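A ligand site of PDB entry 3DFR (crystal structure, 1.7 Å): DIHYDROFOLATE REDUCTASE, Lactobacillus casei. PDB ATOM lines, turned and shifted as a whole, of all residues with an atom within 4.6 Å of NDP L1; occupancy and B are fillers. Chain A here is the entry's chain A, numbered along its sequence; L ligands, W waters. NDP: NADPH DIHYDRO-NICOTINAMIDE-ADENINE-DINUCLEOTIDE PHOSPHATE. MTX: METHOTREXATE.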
ATOM      1  N   TRP A   5      10.464  16.253 -20.736  1.00  0.00           N
ATOM      2  CA  TRP A   5      10.814  16.937 -19.452  1.00  0.00           C
ATOM      3  C   TRP A   5      11.733  15.999 -18.584  1.00  0.00           C
ATOM      4  O   TRP A   5      11.752  14.823 -18.660  1.00  0.00           O
ATOM      5  CB  TRP A   5       9.507  17.468 -18.709  1.00  0.00           C
ATOM      6  CG  TRP A   5       8.779  16.437 -17.935  1.00  0.00           C
ATOM      7  CD1 TRP A   5       8.888  16.241 -16.591  1.00  0.00           C
ATOM      8  CD2 TRP A   5       7.918  15.382 -18.380  1.00  0.00           C
ATOM      9  NE1 TRP A   5       8.006  15.248 -16.093  1.00  0.00           N
ATOM     10  CE2 TRP A   5       7.422  14.737 -17.179  1.00  0.00           C
ATOM     11  CE3 TRP A   5       7.432  15.076 -19.636  1.00  0.00           C
ATOM     12  CZ2 TRP A   5       6.501  13.681 -17.267  1.00  0.00           C
ATOM     13  CZ3 TRP A   5       6.569  14.027 -19.617  1.00  0.00           C
ATOM     14  CH2 TRP A   5       6.020  13.236 -18.518  1.00  0.00           C
ATOM     15  N   ALA A   6      12.291  16.782 -17.586  1.00  0.00           N
ATOM     16  CA  ALA A   6      13.106  16.043 -16.491  1.00  0.00           C
ATOM     17  C   ALA A   6      12.447  16.451 -15.182  1.00  0.00           C
ATOM     18  O   ALA A   6      12.156  17.661 -15.032  1.00  0.00           O
ATOM     19  CB  ALA A   6      14.562  16.561 -16.561  1.00  0.00           C
ATOM     20  N   ILE A  13      10.014  20.283 -11.446  1.00  0.00           N
ATOM     21  CA  ILE A  13      10.713  20.617 -12.657  1.00  0.00           C
ATOM     22  C   ILE A  13      11.504  21.958 -12.752  1.00  0.00           C
ATOM     23  O   ILE A  13      12.366  22.268 -13.548  1.00  0.00           O
ATOM     24  CB  ILE A  13       9.738  20.557 -13.957  1.00  0.00           C
ATOM     25  CG1 ILE A  13       8.714  21.693 -13.883  1.00  0.00           C
ATOM     26  CG2 ILE A  13       9.115  19.087 -14.000  1.00  0.00           C
ATOM     27  CD1 ILE A  13       7.970  21.820 -15.249  1.00  0.00           C
ATOM     28  N   GLY A  14      11.099  22.840 -11.682  1.00  0.00           N
ATOM     29  CA  GLY A  14      11.770  24.173 -11.830  1.00  0.00           C
ATOM     30  C   GLY A  14      11.942  24.910 -10.389  1.00  0.00           C
ATOM     31  O   GLY A  14      11.238  24.542  -9.466  1.00  0.00           O
ATOM     32  N   LYS A  15      12.762  25.956 -10.394  1.00  0.00           N
ATOM     33  CA  LYS A  15      12.988  26.685  -9.207  1.00  0.00           C
ATOM     34  C   LYS A  15      13.396  28.069  -9.676  1.00  0.00           C
ATOM     35  O   LYS A  15      14.398  28.288 -10.470  1.00  0.00           O
ATOM     36  CB  LYS A  15      14.198  26.282  -8.386  1.00  0.00           C
ATOM     37  CG  LYS A  15      14.398  26.953  -6.949  1.00  0.00           C
ATOM     38  CD  LYS A  15      15.680  26.503  -6.248  1.00  0.00           C
ATOM     39  CE  LYS A  15      16.048  26.969  -4.861  1.00  0.00           C
ATOM     40  NZ  LYS A  15      15.190  26.488  -3.665  1.00  0.00           N
ATOM     41  N   GLY A  17      12.544  30.233 -11.910  1.00  0.00           N
ATOM     42  CA  GLY A  17      12.793  30.441 -13.440  1.00  0.00           C
ATOM     43  C   GLY A  17      13.922  29.680 -14.006  1.00  0.00           C
ATOM     44  O   GLY A  17      14.076  29.860 -15.225  1.00  0.00           O
ATOM     45  N   HIS A  18      14.519  28.721 -13.256  1.00  0.00           N
ATOM     46  CA  HIS A  18      15.681  28.031 -13.782  1.00  0.00           C
ATOM     47  C   HIS A  18      15.463  26.530 -13.323  1.00  0.00           C
ATOM     48  O   HIS A  18      14.364  26.160 -12.808  1.00  0.00           O
ATOM     49  CB  HIS A  18      17.095  28.601 -13.220  1.00  0.00           C
ATOM     50  CG  HIS A  18      17.295  28.862 -11.739  1.00  0.00           C
ATOM     51  ND1 HIS A  18      17.700  27.813 -10.714  1.00  0.00           N
ATOM     52  CD2 HIS A  18      17.180  30.011 -10.989  1.00  0.00           C
ATOM     53  CE1 HIS A  18      17.660  28.408  -9.395  1.00  0.00           C
ATOM     54  NE2 HIS A  18      17.423  29.724  -9.421  1.00  0.00           N
ATOM     55  N   LEU A  19      16.322  25.595 -13.620  1.00  0.00           N
ATOM     56  CA  LEU A  19      16.319  24.231 -13.302  1.00  0.00           C
ATOM     57  C   LEU A  19      16.853  24.274 -11.839  1.00  0.00           C
ATOM     58  O   LEU A  19      17.463  24.902 -11.181  1.00  0.00           O
ATOM     59  CB  LEU A  19      17.061  23.223 -14.108  1.00  0.00           C
ATOM     60  CG  LEU A  19      16.569  23.360 -15.582  1.00  0.00           C
ATOM     61  CD1 LEU A  19      17.659  22.578 -16.274  1.00  0.00           C
ATOM     62  CD2 LEU A  19      15.343  22.670 -15.821  1.00  0.00           C
ATOM     63  N   TRP A  21      18.556  21.716 -10.555  1.00  0.00           N
ATOM     64  CA  TRP A  21      19.717  20.846 -10.587  1.00  0.00           C
ATOM     65  C   TRP A  21      20.508  21.390 -11.816  1.00  0.00           C
ATOM     66  O   TRP A  21      20.065  22.016 -12.782  1.00  0.00           O
ATOM     67  CB  TRP A  21      19.445  19.350 -10.599  1.00  0.00           C
ATOM     68  CG  TRP A  21      18.639  19.077 -11.898  1.00  0.00           C
ATOM     69  CD1 TRP A  21      18.794  19.011 -13.272  1.00  0.00           C
ATOM     70  CD2 TRP A  21      17.143  18.922 -11.673  1.00  0.00           C
ATOM     71  NE1 TRP A  21      17.609  18.899 -13.898  1.00  0.00           N
ATOM     72  CE2 TRP A  21      16.575  18.771 -13.011  1.00  0.00           C
ATOM     73  CE3 TRP A  21      16.253  18.773 -10.510  1.00  0.00           C
ATOM     74  CZ2 TRP A  21      15.203  18.672 -13.293  1.00  0.00           C
ATOM     75  CZ3 TRP A  21      14.900  18.542 -10.820  1.00  0.00           C
ATOM     76  CH2 TRP A  21      14.424  18.474 -12.143  1.00  0.00           C
ATOM     77  N   GLY A  42       7.406  27.745 -23.684  1.00  0.00           N
ATOM     78  CA  GLY A  42       6.774  28.948 -23.107  1.00  0.00           C
ATOM     79  C   GLY A  42       7.864  29.990 -23.049  1.00  0.00           C
ATOM     80  O   GLY A  42       9.134  29.853 -23.036  1.00  0.00           O
ATOM     81  N   ARG A  43       7.428  31.297 -23.102  1.00  0.00           N
ATOM     82  CA  ARG A  43       8.278  32.453 -23.171  1.00  0.00           C
ATOM     83  C   ARG A  43       9.355  32.380 -21.983  1.00  0.00           C
ATOM     84  O   ARG A  43      10.527  32.794 -22.185  1.00  0.00           O
ATOM     85  CB  ARG A  43       7.467  33.713 -23.234  1.00  0.00           C
ATOM     86  CG  ARG A  43       8.379  34.952 -23.337  1.00  0.00           C
ATOM     87  CD  ARG A  43       8.884  35.658 -22.115  1.00  0.00           C
ATOM     88  NE  ARG A  43       7.796  35.897 -21.083  1.00  0.00           N
ATOM     89  CZ  ARG A  43       8.081  36.107 -19.733  1.00  0.00           C
ATOM     90  NH1 ARG A  43       9.377  36.022 -19.365  1.00  0.00           N
ATOM     91  NH2 ARG A  43       7.026  36.116 -18.899  1.00  0.00           N
ATOM     92  N   ARG A  44       8.744  32.105 -20.725  1.00  0.00           N
ATOM     93  CA  ARG A  44       9.806  32.110 -19.655  1.00  0.00           C
ATOM     94  C   ARG A  44      10.832  31.106 -19.714  1.00  0.00           C
ATOM     95  O   ARG A  44      12.026  31.291 -19.490  1.00  0.00           O
ATOM     96  CB  ARG A  44       8.742  31.934 -18.498  1.00  0.00           C
ATOM     97  CG  ARG A  44       9.136  32.161 -17.047  1.00  0.00           C
ATOM     98  CD  ARG A  44       7.687  32.237 -16.467  1.00  0.00           C
ATOM     99  NE  ARG A  44       6.980  33.181 -15.878  1.00  0.00           N
ATOM    100  CZ  ARG A  44       5.760  33.023 -15.287  1.00  0.00           C
ATOM    101  NH1 ARG A  44       5.221  31.787 -14.756  1.00  0.00           N
ATOM    102  NH2 ARG A  44       5.118  34.270 -15.199  1.00  0.00           N
ATOM    103  N   THR A  45      10.566  29.859 -20.137  1.00  0.00           N
ATOM    104  CA  THR A  45      11.581  28.741 -20.374  1.00  0.00           C
ATOM    105  C   THR A  45      12.356  29.379 -21.643  1.00  0.00           C
ATOM    106  O   THR A  45      13.583  29.224 -21.494  1.00  0.00           O
ATOM    107  CB  THR A  45      10.963  27.374 -20.882  1.00  0.00           C
ATOM    108  OG1 THR A  45      10.207  27.136 -19.658  1.00  0.00           O
ATOM    109  CG2 THR A  45      11.951  26.307 -21.345  1.00  0.00           C
ATOM    110  N   LEU A  62       5.830  30.507 -27.347  1.00  0.00           N
ATOM    111  CA  LEU A  62       4.373  30.792 -27.101  1.00  0.00           C
ATOM    112  C   LEU A  62       4.312  32.002 -26.109  1.00  0.00           C
ATOM    113  O   LEU A  62       4.950  32.060 -25.038  1.00  0.00           O
ATOM    114  CB  LEU A  62       3.375  29.773 -26.442  1.00  0.00           C
ATOM    115  CG  LEU A  62       2.921  28.671 -27.332  1.00  0.00           C
ATOM    116  CD1 LEU A  62       1.838  27.806 -26.593  1.00  0.00           C
ATOM    117  CD2 LEU A  62       1.740  29.687 -27.939  1.00  0.00           C
ATOM    118  N   THR A  63       3.787  33.277 -26.354  1.00  0.00           N
ATOM    119  CA  THR A  63       3.910  34.462 -25.522  1.00  0.00           C
ATOM    120  C   THR A  63       2.554  35.254 -25.540  1.00  0.00           C
ATOM    121  O   THR A  63       1.960  35.028 -26.706  1.00  0.00           O
ATOM    122  CB  THR A  63       5.088  35.450 -25.857  1.00  0.00           C
ATOM    123  OG1 THR A  63       4.866  36.509 -24.909  1.00  0.00           O
ATOM    124  CG2 THR A  63       5.112  35.725 -27.441  1.00  0.00           C
ATOM    125  N   HIS A  64       1.906  35.909 -24.691  1.00  0.00           N
ATOM    126  CA  HIS A  64       0.697  36.691 -24.990  1.00  0.00           C
ATOM    127  C   HIS A  64       1.049  38.137 -25.411  1.00  0.00           C
ATOM    128  O   HIS A  64       0.061  38.861 -25.828  1.00  0.00           O
ATOM    129  CB  HIS A  64      -0.092  36.845 -23.614  1.00  0.00           C
ATOM    130  CG  HIS A  64      -0.706  35.578 -23.357  1.00  0.00           C
ATOM    131  ND1 HIS A  64      -1.536  34.840 -23.959  1.00  0.00           N
ATOM    132  CD2 HIS A  64      -0.329  35.023 -22.112  1.00  0.00           C
ATOM    133  CE1 HIS A  64      -1.971  33.731 -23.216  1.00  0.00           C
ATOM    134  NE2 HIS A  64      -1.135  33.829 -22.162  1.00  0.00           N
ATOM    135  N   GLN A  65       2.424  38.403 -25.307  1.00  0.00           N
ATOM    136  CA  GLN A  65       2.933  39.780 -25.580  1.00  0.00           C
ATOM    137  C   GLN A  65       2.795  39.938 -27.049  1.00  0.00           C
ATOM    138  O   GLN A  65       3.606  39.282 -27.838  1.00  0.00           O
ATOM    139  CB  GLN A  65       4.262  40.101 -25.117  1.00  0.00           C
ATOM    140  CG  GLN A  65       4.534  39.649 -23.654  1.00  0.00           C
ATOM    141  CD  GLN A  65       5.935  40.163 -23.267  1.00  0.00           C
ATOM    142  OE1 GLN A  65       6.558  41.083 -23.830  1.00  0.00           O
ATOM    143  NE2 GLN A  65       6.385  38.999 -22.445  1.00  0.00           N
ATOM    144  N   HIS A  77       1.104  33.110 -30.526  1.00  0.00           N
ATOM    145  CA  HIS A  77       0.283  33.605 -29.407  1.00  0.00           C
ATOM    146  C   HIS A  77      -0.831  32.748 -28.949  1.00  0.00           C
ATOM    147  O   HIS A  77      -1.520  33.157 -28.041  1.00  0.00           O
ATOM    148  CB  HIS A  77      -0.239  35.183 -29.553  1.00  0.00           C
ATOM    149  CG  HIS A  77       0.744  36.143 -30.074  1.00  0.00           C
ATOM    150  ND1 HIS A  77       1.883  36.599 -29.522  1.00  0.00           N
ATOM    151  CD2 HIS A  77       0.993  36.444 -31.433  1.00  0.00           C
ATOM    152  CE1 HIS A  77       2.701  37.392 -30.276  1.00  0.00           C
ATOM    153  NE2 HIS A  77       2.016  37.256 -31.537  1.00  0.00           N
ATOM    154  N   ASP A  78      -0.971  31.568 -29.538  1.00  0.00           N
ATOM    155  CA  ASP A  78      -2.082  30.708 -28.980  1.00  0.00           C
ATOM    156  C   ASP A  78      -1.661  29.374 -29.357  1.00  0.00           C
ATOM    157  O   ASP A  78      -0.858  29.142 -30.453  1.00  0.00           O
ATOM    158  CB  ASP A  78      -3.314  31.409 -29.570  1.00  0.00           C
ATOM    159  CG  ASP A  78      -3.832  31.624 -30.870  1.00  0.00           C
ATOM    160  OD1 ASP A  78      -3.315  30.719 -31.733  1.00  0.00           O
ATOM    161  OD2 ASP A  78      -4.882  32.572 -30.712  1.00  0.00           O
ATOM    162  N   VAL A  79      -2.274  28.247 -28.974  1.00  0.00           N
ATOM    163  CA  VAL A  79      -2.054  26.878 -29.415  1.00  0.00           C
ATOM    164  C   VAL A  79      -2.457  26.586 -30.879  1.00  0.00           C
ATOM    165  O   VAL A  79      -1.707  25.865 -31.535  1.00  0.00           O
ATOM    166  CB  VAL A  79      -2.893  25.939 -28.341  1.00  0.00           C
ATOM    167  CG1 VAL A  79      -2.919  24.595 -28.739  1.00  0.00           C
ATOM    168  CG2 VAL A  79      -2.044  25.999 -27.093  1.00  0.00           C
ATOM    169  N   ALA A  97       8.410  21.211 -24.898  1.00  0.00           N
ATOM    170  CA  ALA A  97       9.515  21.142 -23.934  1.00  0.00           C
ATOM    171  C   ALA A  97       9.241  22.005 -22.599  1.00  0.00           C
ATOM    172  O   ALA A  97      10.257  22.003 -21.899  1.00  0.00           O
ATOM    173  CB  ALA A  97      10.763  21.549 -24.765  1.00  0.00           C
ATOM    174  N   GLY A  98       8.049  22.500 -22.403  1.00  0.00           N
ATOM    175  CA  GLY A  98       7.776  23.213 -21.223  1.00  0.00           C
ATOM    176  C   GLY A  98       7.697  24.674 -21.254  1.00  0.00           C
ATOM    177  O   GLY A  98       7.934  25.144 -22.278  1.00  0.00           O
ATOM    178  N   GLY A  99       7.478  25.329 -20.021  1.00  0.00           N
ATOM    179  CA  GLY A  99       7.374  24.699 -18.746  1.00  0.00           C
ATOM    180  C   GLY A  99       6.034  24.380 -18.554  1.00  0.00           C
ATOM    181  O   GLY A  99       5.213  23.956 -19.322  1.00  0.00           O
ATOM    182  N   ALA A 100       5.565  24.387 -17.234  1.00  0.00           N
ATOM    183  CA  ALA A 100       4.282  23.948 -16.730  1.00  0.00           C
ATOM    184  C   ALA A 100       2.979  24.551 -17.416  1.00  0.00           C
ATOM    185  O   ALA A 100       2.039  23.804 -17.818  1.00  0.00           O
ATOM    186  CB  ALA A 100       4.126  24.106 -15.205  1.00  0.00           C
ATOM    187  N   GLN A 101       3.080  25.886 -17.658  1.00  0.00           N
ATOM    188  CA  GLN A 101       1.882  26.524 -18.273  1.00  0.00           C
ATOM    189  C   GLN A 101       1.766  25.955 -19.676  1.00  0.00           C
ATOM    190  O   GLN A 101       0.700  25.747 -20.209  1.00  0.00           O
ATOM    191  CB  GLN A 101       2.149  27.985 -18.559  1.00  0.00           C
ATOM    192  CG  GLN A 101       1.932  28.498 -17.170  1.00  0.00           C
ATOM    193  CD  GLN A 101       1.872  30.016 -17.239  1.00  0.00           C
ATOM    194  OE1 GLN A 101       2.347  30.724 -16.419  1.00  0.00           O
ATOM    195  NE2 GLN A 101       1.359  30.658 -18.202  1.00  0.00           N
ATOM    196  N   ILE A 102       2.916  25.742 -20.383  1.00  0.00           N
ATOM    197  CA  ILE A 102       2.715  25.121 -21.764  1.00  0.00           C
ATOM    198  C   ILE A 102       2.394  23.700 -21.801  1.00  0.00           C
ATOM    199  O   ILE A 102       1.601  23.320 -22.687  1.00  0.00           O
ATOM    200  CB  ILE A 102       4.095  25.436 -22.564  1.00  0.00           C
ATOM    201  CG1 ILE A 102       4.180  26.652 -23.396  1.00  0.00           C
ATOM    202  CG2 ILE A 102       4.619  24.510 -23.647  1.00  0.00           C
ATOM    203  CD1 ILE A 102       3.440  27.857 -22.823  1.00  0.00           C
ATOM    204  N   ALA A 105      -1.282  23.788 -21.541  1.00  0.00           N
ATOM    205  CA  ALA A 105      -1.972  24.227 -22.834  1.00  0.00           C
ATOM    206  C   ALA A 105      -1.847  23.034 -23.620  1.00  0.00           C
ATOM    207  O   ALA A 105      -2.939  22.869 -24.509  1.00  0.00           O
ATOM    208  CB  ALA A 105      -1.022  25.363 -23.402  1.00  0.00           C
ATOM    209  N   THR A 126       8.069  24.661  -9.081  1.00  0.00           N
ATOM    210  CA  THR A 126       7.209  24.360 -10.283  1.00  0.00           C
ATOM    211  C   THR A 126       7.333  22.800 -10.374  1.00  0.00           C
ATOM    212  O   THR A 126       8.407  22.284 -10.308  1.00  0.00           O
ATOM    213  CB  THR A 126       7.816  25.065 -11.618  1.00  0.00           C
ATOM    214  OG1 THR A 126       7.822  26.402 -11.128  1.00  0.00           O
ATOM    215  CG2 THR A 126       6.907  24.830 -12.793  1.00  0.00           C
HETATM  216  PA  NDP L   1       6.490  28.561 -19.177  1.00  0.00           P
HETATM  217  O1A NDP L   1       5.435  27.542 -19.401  1.00  0.00           O
HETATM  218  O2A NDP L   1       7.851  28.248 -19.655  1.00  0.00           O
HETATM  219  O5B NDP L   1       6.143  30.081 -19.711  1.00  0.00           O
HETATM  220  C5B NDP L   1       4.816  30.758 -19.426  1.00  0.00           C
HETATM  221  C4B NDP L   1       4.698  31.974 -20.447  1.00  0.00           C
HETATM  222  O4B NDP L   1       4.192  31.329 -21.473  1.00  0.00           O
HETATM  223  C3B NDP L   1       3.447  32.810 -19.911  1.00  0.00           C
HETATM  224  O3B NDP L   1       4.119  33.678 -18.910  1.00  0.00           O
HETATM  225  C2B NDP L   1       3.170  33.365 -21.384  1.00  0.00           C
HETATM  226  O2B NDP L   1       4.213  34.295 -21.674  1.00  0.00           O
HETATM  227  C1B NDP L   1       3.241  32.146 -22.255  1.00  0.00           C
HETATM  228  N9A NDP L   1       2.022  31.424 -22.320  1.00  0.00           N
HETATM  229  C8A NDP L   1       1.465  30.490 -21.507  1.00  0.00           C
HETATM  230  N7A NDP L   1       0.462  29.813 -21.883  1.00  0.00           N
HETATM  231  C5A NDP L   1       0.078  30.570 -23.038  1.00  0.00           C
HETATM  232  C6A NDP L   1      -1.049  30.289 -24.103  1.00  0.00           C
HETATM  233  N6A NDP L   1      -1.954  29.318 -23.950  1.00  0.00           N
HETATM  234  N1A NDP L   1      -0.866  31.046 -25.094  1.00  0.00           N
HETATM  235  C2A NDP L   1       0.226  31.911 -25.228  1.00  0.00           C
HETATM  236  N3A NDP L   1       1.207  32.323 -24.379  1.00  0.00           N
HETATM  237  C4A NDP L   1       1.131  31.388 -23.326  1.00  0.00           C
HETATM  238  O3  NDP L   1       6.692  28.909 -17.635  1.00  0.00           O
HETATM  239  PN  NDP L   1       6.297  28.200 -16.242  1.00  0.00           P
HETATM  240  O1N NDP L   1       5.105  27.402 -16.280  1.00  0.00           O
HETATM  241  O2N NDP L   1       6.794  29.174 -15.171  1.00  0.00           O
HETATM  242  O5D NDP L   1       7.594  27.193 -16.238  1.00  0.00           O
HETATM  243  C5D NDP L   1       9.050  27.582 -16.294  1.00  0.00           C
HETATM  244  C4D NDP L   1       9.668  26.796 -15.111  1.00  0.00           C
HETATM  245  O4D NDP L   1       9.754  25.387 -15.589  1.00  0.00           O
HETATM  246  C3D NDP L   1      11.127  27.251 -14.922  1.00  0.00           C
HETATM  247  O3D NDP L   1      11.617  27.009 -13.598  1.00  0.00           O
HETATM  248  C2D NDP L   1      11.846  26.290 -15.863  1.00  0.00           C
HETATM  249  O2D NDP L   1      13.241  26.163 -15.477  1.00  0.00           O
HETATM  250  C1D NDP L   1      11.098  24.969 -15.702  1.00  0.00           C
HETATM  251  N1N NDP L   1      11.346  23.883 -16.760  1.00  0.00           N
HETATM  252  C2N NDP L   1      11.882  22.679 -16.635  1.00  0.00           C
HETATM  253  C3N NDP L   1      11.710  21.678 -17.432  1.00  0.00           C
HETATM  254  C7N NDP L   1      12.426  20.554 -16.914  1.00  0.00           C
HETATM  255  O7N NDP L   1      12.248  19.646 -17.853  1.00  0.00           O
HETATM  256  N7N NDP L   1      12.764  20.261 -15.635  1.00  0.00           N
HETATM  257  C4N NDP L   1      11.334  22.046 -18.829  1.00  0.00           C
HETATM  258  C5N NDP L   1      10.924  23.404 -19.070  1.00  0.00           C
HETATM  259  C6N NDP L   1      10.904  24.358 -18.063  1.00  0.00           C
HETATM  260  P2B NDP L   1       4.133  35.962 -21.637  1.00  0.00           P
HETATM  261  O1X NDP L   1       5.446  36.313 -22.335  1.00  0.00           O
HETATM  262  O2X NDP L   1       2.672  36.179 -22.019  1.00  0.00           O
HETATM  263  O3X NDP L   1       4.302  36.138 -20.075  1.00  0.00           O
HETATM  264  N1  MTX L   2      15.649  18.216 -19.855  1.00  0.00           N
HETATM  265  C2  MTX L   2      14.633  17.456 -20.442  1.00  0.00           C
HETATM  266  NA2 MTX L   2      14.823  16.099 -20.429  1.00  0.00           N
HETATM  267  N3  MTX L   2      13.526  18.029 -20.946  1.00  0.00           N
HETATM  268  C4  MTX L   2      13.268  19.361 -21.053  1.00  0.00           C
HETATM  269  NA4 MTX L   2      12.202  19.898 -21.596  1.00  0.00           N
HETATM  270  C4A MTX L   2      14.364  20.192 -20.509  1.00  0.00           C
HETATM  271  N5  MTX L   2      14.312  21.535 -20.620  1.00  0.00           N
HETATM  272  C6  MTX L   2      15.335  22.212 -20.095  1.00  0.00           C
HETATM  273  C7  MTX L   2      16.339  21.489 -19.457  1.00  0.00           C
HETATM  274  N8  MTX L   2      16.521  20.297 -19.361  1.00  0.00           N
HETATM  275  C8A MTX L   2      15.480  19.574 -19.880  1.00  0.00           C
HETATM  276  C9  MTX L   2      15.127  23.737 -20.085  1.00  0.00           C
HETATM  277  N10 MTX L   2      16.320  24.417 -20.045  1.00  0.00           N
HETATM  278  CM  MTX L   2      16.378  25.395 -18.884  1.00  0.00           C
HETATM  279  C11 MTX L   2      19.533  24.056 -22.674  1.00  0.00           C
HETATM  280  C12 MTX L   2      19.688  24.731 -21.477  1.00  0.00           C
HETATM  281  C13 MTX L   2      18.802  25.033 -20.495  1.00  0.00           C
HETATM  282  C14 MTX L   2      17.428  24.408 -20.842  1.00  0.00           C
HETATM  283  C15 MTX L   2      17.354  23.593 -22.079  1.00  0.00           C
HETATM  284  C16 MTX L   2      18.325  23.344 -22.881  1.00  0.00           C
HETATM  285  C   MTX L   2      20.640  23.902 -23.345  1.00  0.00           C
HETATM  286  O   MTX L   2      21.766  24.394 -23.360  1.00  0.00           O
HETATM  287  N   MTX L   2      20.957  22.912 -24.145  1.00  0.00           N
HETATM  288  CA  MTX L   2      21.742  22.564 -25.207  1.00  0.00           C
HETATM  289  CT  MTX L   2      20.898  22.144 -26.397  1.00  0.00           C
HETATM  290  O1  MTX L   2      19.844  21.545 -26.525  1.00  0.00           O
HETATM  291  O2  MTX L   2      21.663  22.311 -27.533  1.00  0.00           O
HETATM  292  CB  MTX L   2      22.796  21.391 -25.230  1.00  0.00           C
HETATM  293  CG  MTX L   2      24.028  21.485 -24.413  1.00  0.00           C
HETATM  294  CD  MTX L   2      24.875  20.440 -23.428  1.00  0.00           C
HETATM  295  OE1 MTX L   2      25.708  20.840 -22.417  1.00  0.00           O
HETATM  296  OE2 MTX L   2      24.626  19.535 -24.362  1.00  0.00           O
HETATM  297  O   HOH W   1       6.167  28.347 -12.319  1.00  0.00           O
HETATM  298  O   HOH W   2       8.599  30.137 -13.477  1.00  0.00           O
HETATM  299  O   HOH W   3       0.999  36.065 -19.539  1.00  0.00           O
HETATM  300  O   HOH W   4       2.559  33.825 -16.415  1.00  0.00           O
HETATM  301  O   HOH W   5      -3.389  32.449 -25.716  1.00  0.00           O
HETATM  302  O   HOH W   6      13.504  26.484 -18.432  1.00  0.00           O
HETATM  303  O   HOH W   7      -4.402  29.026 -26.208  1.00  0.00           O
HETATM  304  O   HOH W   8       1.645  38.466 -21.322  1.00  0.00           O
HETATM  305  O   HOH W   9      -4.384  27.486 -23.422  1.00  0.00           O
HETATM  306  O   HOH W  10       3.843  27.736 -13.966  1.00  0.00           O
HETATM  307  O   HOH W  11      10.318  28.452 -11.663  1.00  0.00           O
HETATM  308  O   HOH W  12      -1.314  27.836 -20.303  1.00  0.00           O
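The backbone NH (N) of Gly 99 is in hydrogen-bond range of the side-chain hydroxyl (OG1) of Thr 45, at 3.3 Å.
The side-chain hydroxyl of Thr 63 is in hydrogen-bond range of the backbone NH of Gln 65, 3.1 Å away.
O of Thr 63 lies within hydrogen-bond range of ND1 of His 77 (3.2 Å).
O of Leu 62 sits at hydrogen-bond distance from N of Arg 43.
OE1 of Gln 101 sits at hydrogen-bond distance from NH1 of Arg 44, at 3.5 Å.
The backbone NH (N) of Ile 13 sits at hydrogen-bond distance from the backbone carbonyl oxygen (O) of Thr 126, 2.8 Å away.
The backbone carbonyl oxygen (O) of Thr 126 is in hydrogen-bond range of the backbone NH (N) of Gly 14, at 3.1 Å.
The backbone carbonyl oxygen of Gly 98 lies within hydrogen-bond range of the backbone NH of Gly 42 (3.0 Å).
Trp 5 touches NDP L1.
Gly 14 touches NDP L1.
Lys 15 touches NDP L1.
Gly 17 touches NDP L1.
CD2 of Leu 19 touches N7N of NDP L1 (3.5 Å).
CZ2 of Trp 21 touches N7N of NDP L1, 3.7 Å away.
Gly 42 touches NDP L1.
Leu 62 touches NDP L1.
O of His 77 touches C2A of NDP L1, at 3.5 Å.
Ala 97 touches NDP L1 (O to C5N, 3.2 Å).
Gly 98 touches NDP L1 (CA to C5N, 3.8 Å).
Hydrophobic or aromatic side chains that line NDP L1: Trp 5, Ile 13, Leu 19, Trp 21, Leu 62, His 64, Ala 100 and Ile 102.
Within 4 Å of NDP L1: Trp 5, Ala 6, Ile 13, Gly 14, Lys 15, Gly 17, His 18, Leu 19, Trp 21, Gly 42, Arg 43, Arg 44, Thr 45, Leu 62, Thr 63, His 64, Gln 65, His 77, Ala 97, Gly 98, Gly 99, Ala 100, Gln 101 and Ile 102.
An oxygen (O2A) of NDP L1 is in hydrogen-bond range of the backbone NH (N) of Thr 45 (3.2 Å).
An oxygen (O2A) of NDP L1 lies within hydrogen-bond range of the side-chain hydroxyl (OG1) of Thr 45 (2.6 Å).
A nitrogen (N3A) of NDP L1 is in hydrogen-bond range of the backbone NH (N) of Thr 63.
The side-chain hydroxyl (OG1) of Thr 63 lies within hydrogen-bond range of an oxygen (O1X) of NDP L1 (2.6 Å).
NE of Arg 43 is in salt-bridge range of O1X of NDP L1 (2.7 Å).
N of Ala 6 is in hydrogen-bond range of O7N of NDP L1 (2.9 Å).
The backbone carbonyl oxygen (O) of Ala 6 is in hydrogen-bond range of a nitrogen (N7N) of NDP L1.
An oxygen (O2X) of NDP L1 sits at hydrogen-bond distance from the backbone NH (N) of His 64, 2.8 Å away.
NE2 of Gln 65 lies within hydrogen-bond range of O1X of NDP L1, 2.8 Å away.
The backbone NH (N) of Gln 101 sits at hydrogen-bond distance from an oxygen (O1N) of NDP L1, at 2.9 Å.
An oxygen (O3D) of NDP L1 lies within hydrogen-bond range of the backbone NH of His 18 (3.4 Å).
The backbone carbonyl oxygen of His 18 sits at hydrogen-bond distance from an oxygen (O2D) of NDP L1.
The backbone carbonyl oxygen (O) of Ile 13 sits at hydrogen-bond distance from a nitrogen (N7N) of NDP L1 (2.9 Å).
The backbone NH (N) of Gly 99 sits at hydrogen-bond distance from an oxygen (O2A) of NDP L1 (3.0 Å).
The backbone NH of Arg 44 lies close to an oxygen (O5B) of NDP L1 (3.4 Å).
An oxygen (O2N) of NDP L1 is in salt-bridge range of the guanidinium group (NH1) of Arg 44 (3.1 Å).
N of Ala 100 is in hydrogen-bond range of O1N of NDP L1 (3.2 Å).
An oxygen (O1A) of NDP L1 lies within hydrogen-bond range of the backbone NH of Ile 102.
The backbone carbonyl oxygen of Ala 97 lies within hydrogen-bond range of a nitrogen (NA4) of MTX L2, at 2.9 Å.
Water W11 lies within hydrogen-bond range of an oxygen (O3D) of NDP L1, the backbone NH of Gly 17 and the side-chain hydroxyl of Thr 126.
Water W4 lies within hydrogen-bond range of NH2 of Arg 44 (2.9 Å), O3B of NDP L1 (2.9 Å) and OE1 of Gln 101 (3.1 Å).
Water W5 lies within hydrogen-bond range of N1A of NDP L1 (3.0 Å), O of His 77 (3.1 Å) and ND1 of His 64 (3.5 Å).
Water W1 bridges the side-chain hydroxyl (OG1) of Thr 126 (2.8 Å) and an oxygen (O2N) of NDP L1 (3.0 Å).
Water W12 bridges the backbone carbonyl oxygen (O) of Gln 101 (2.9 Å) and a nitrogen (N7A) of NDP L1 (3.1 Å).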
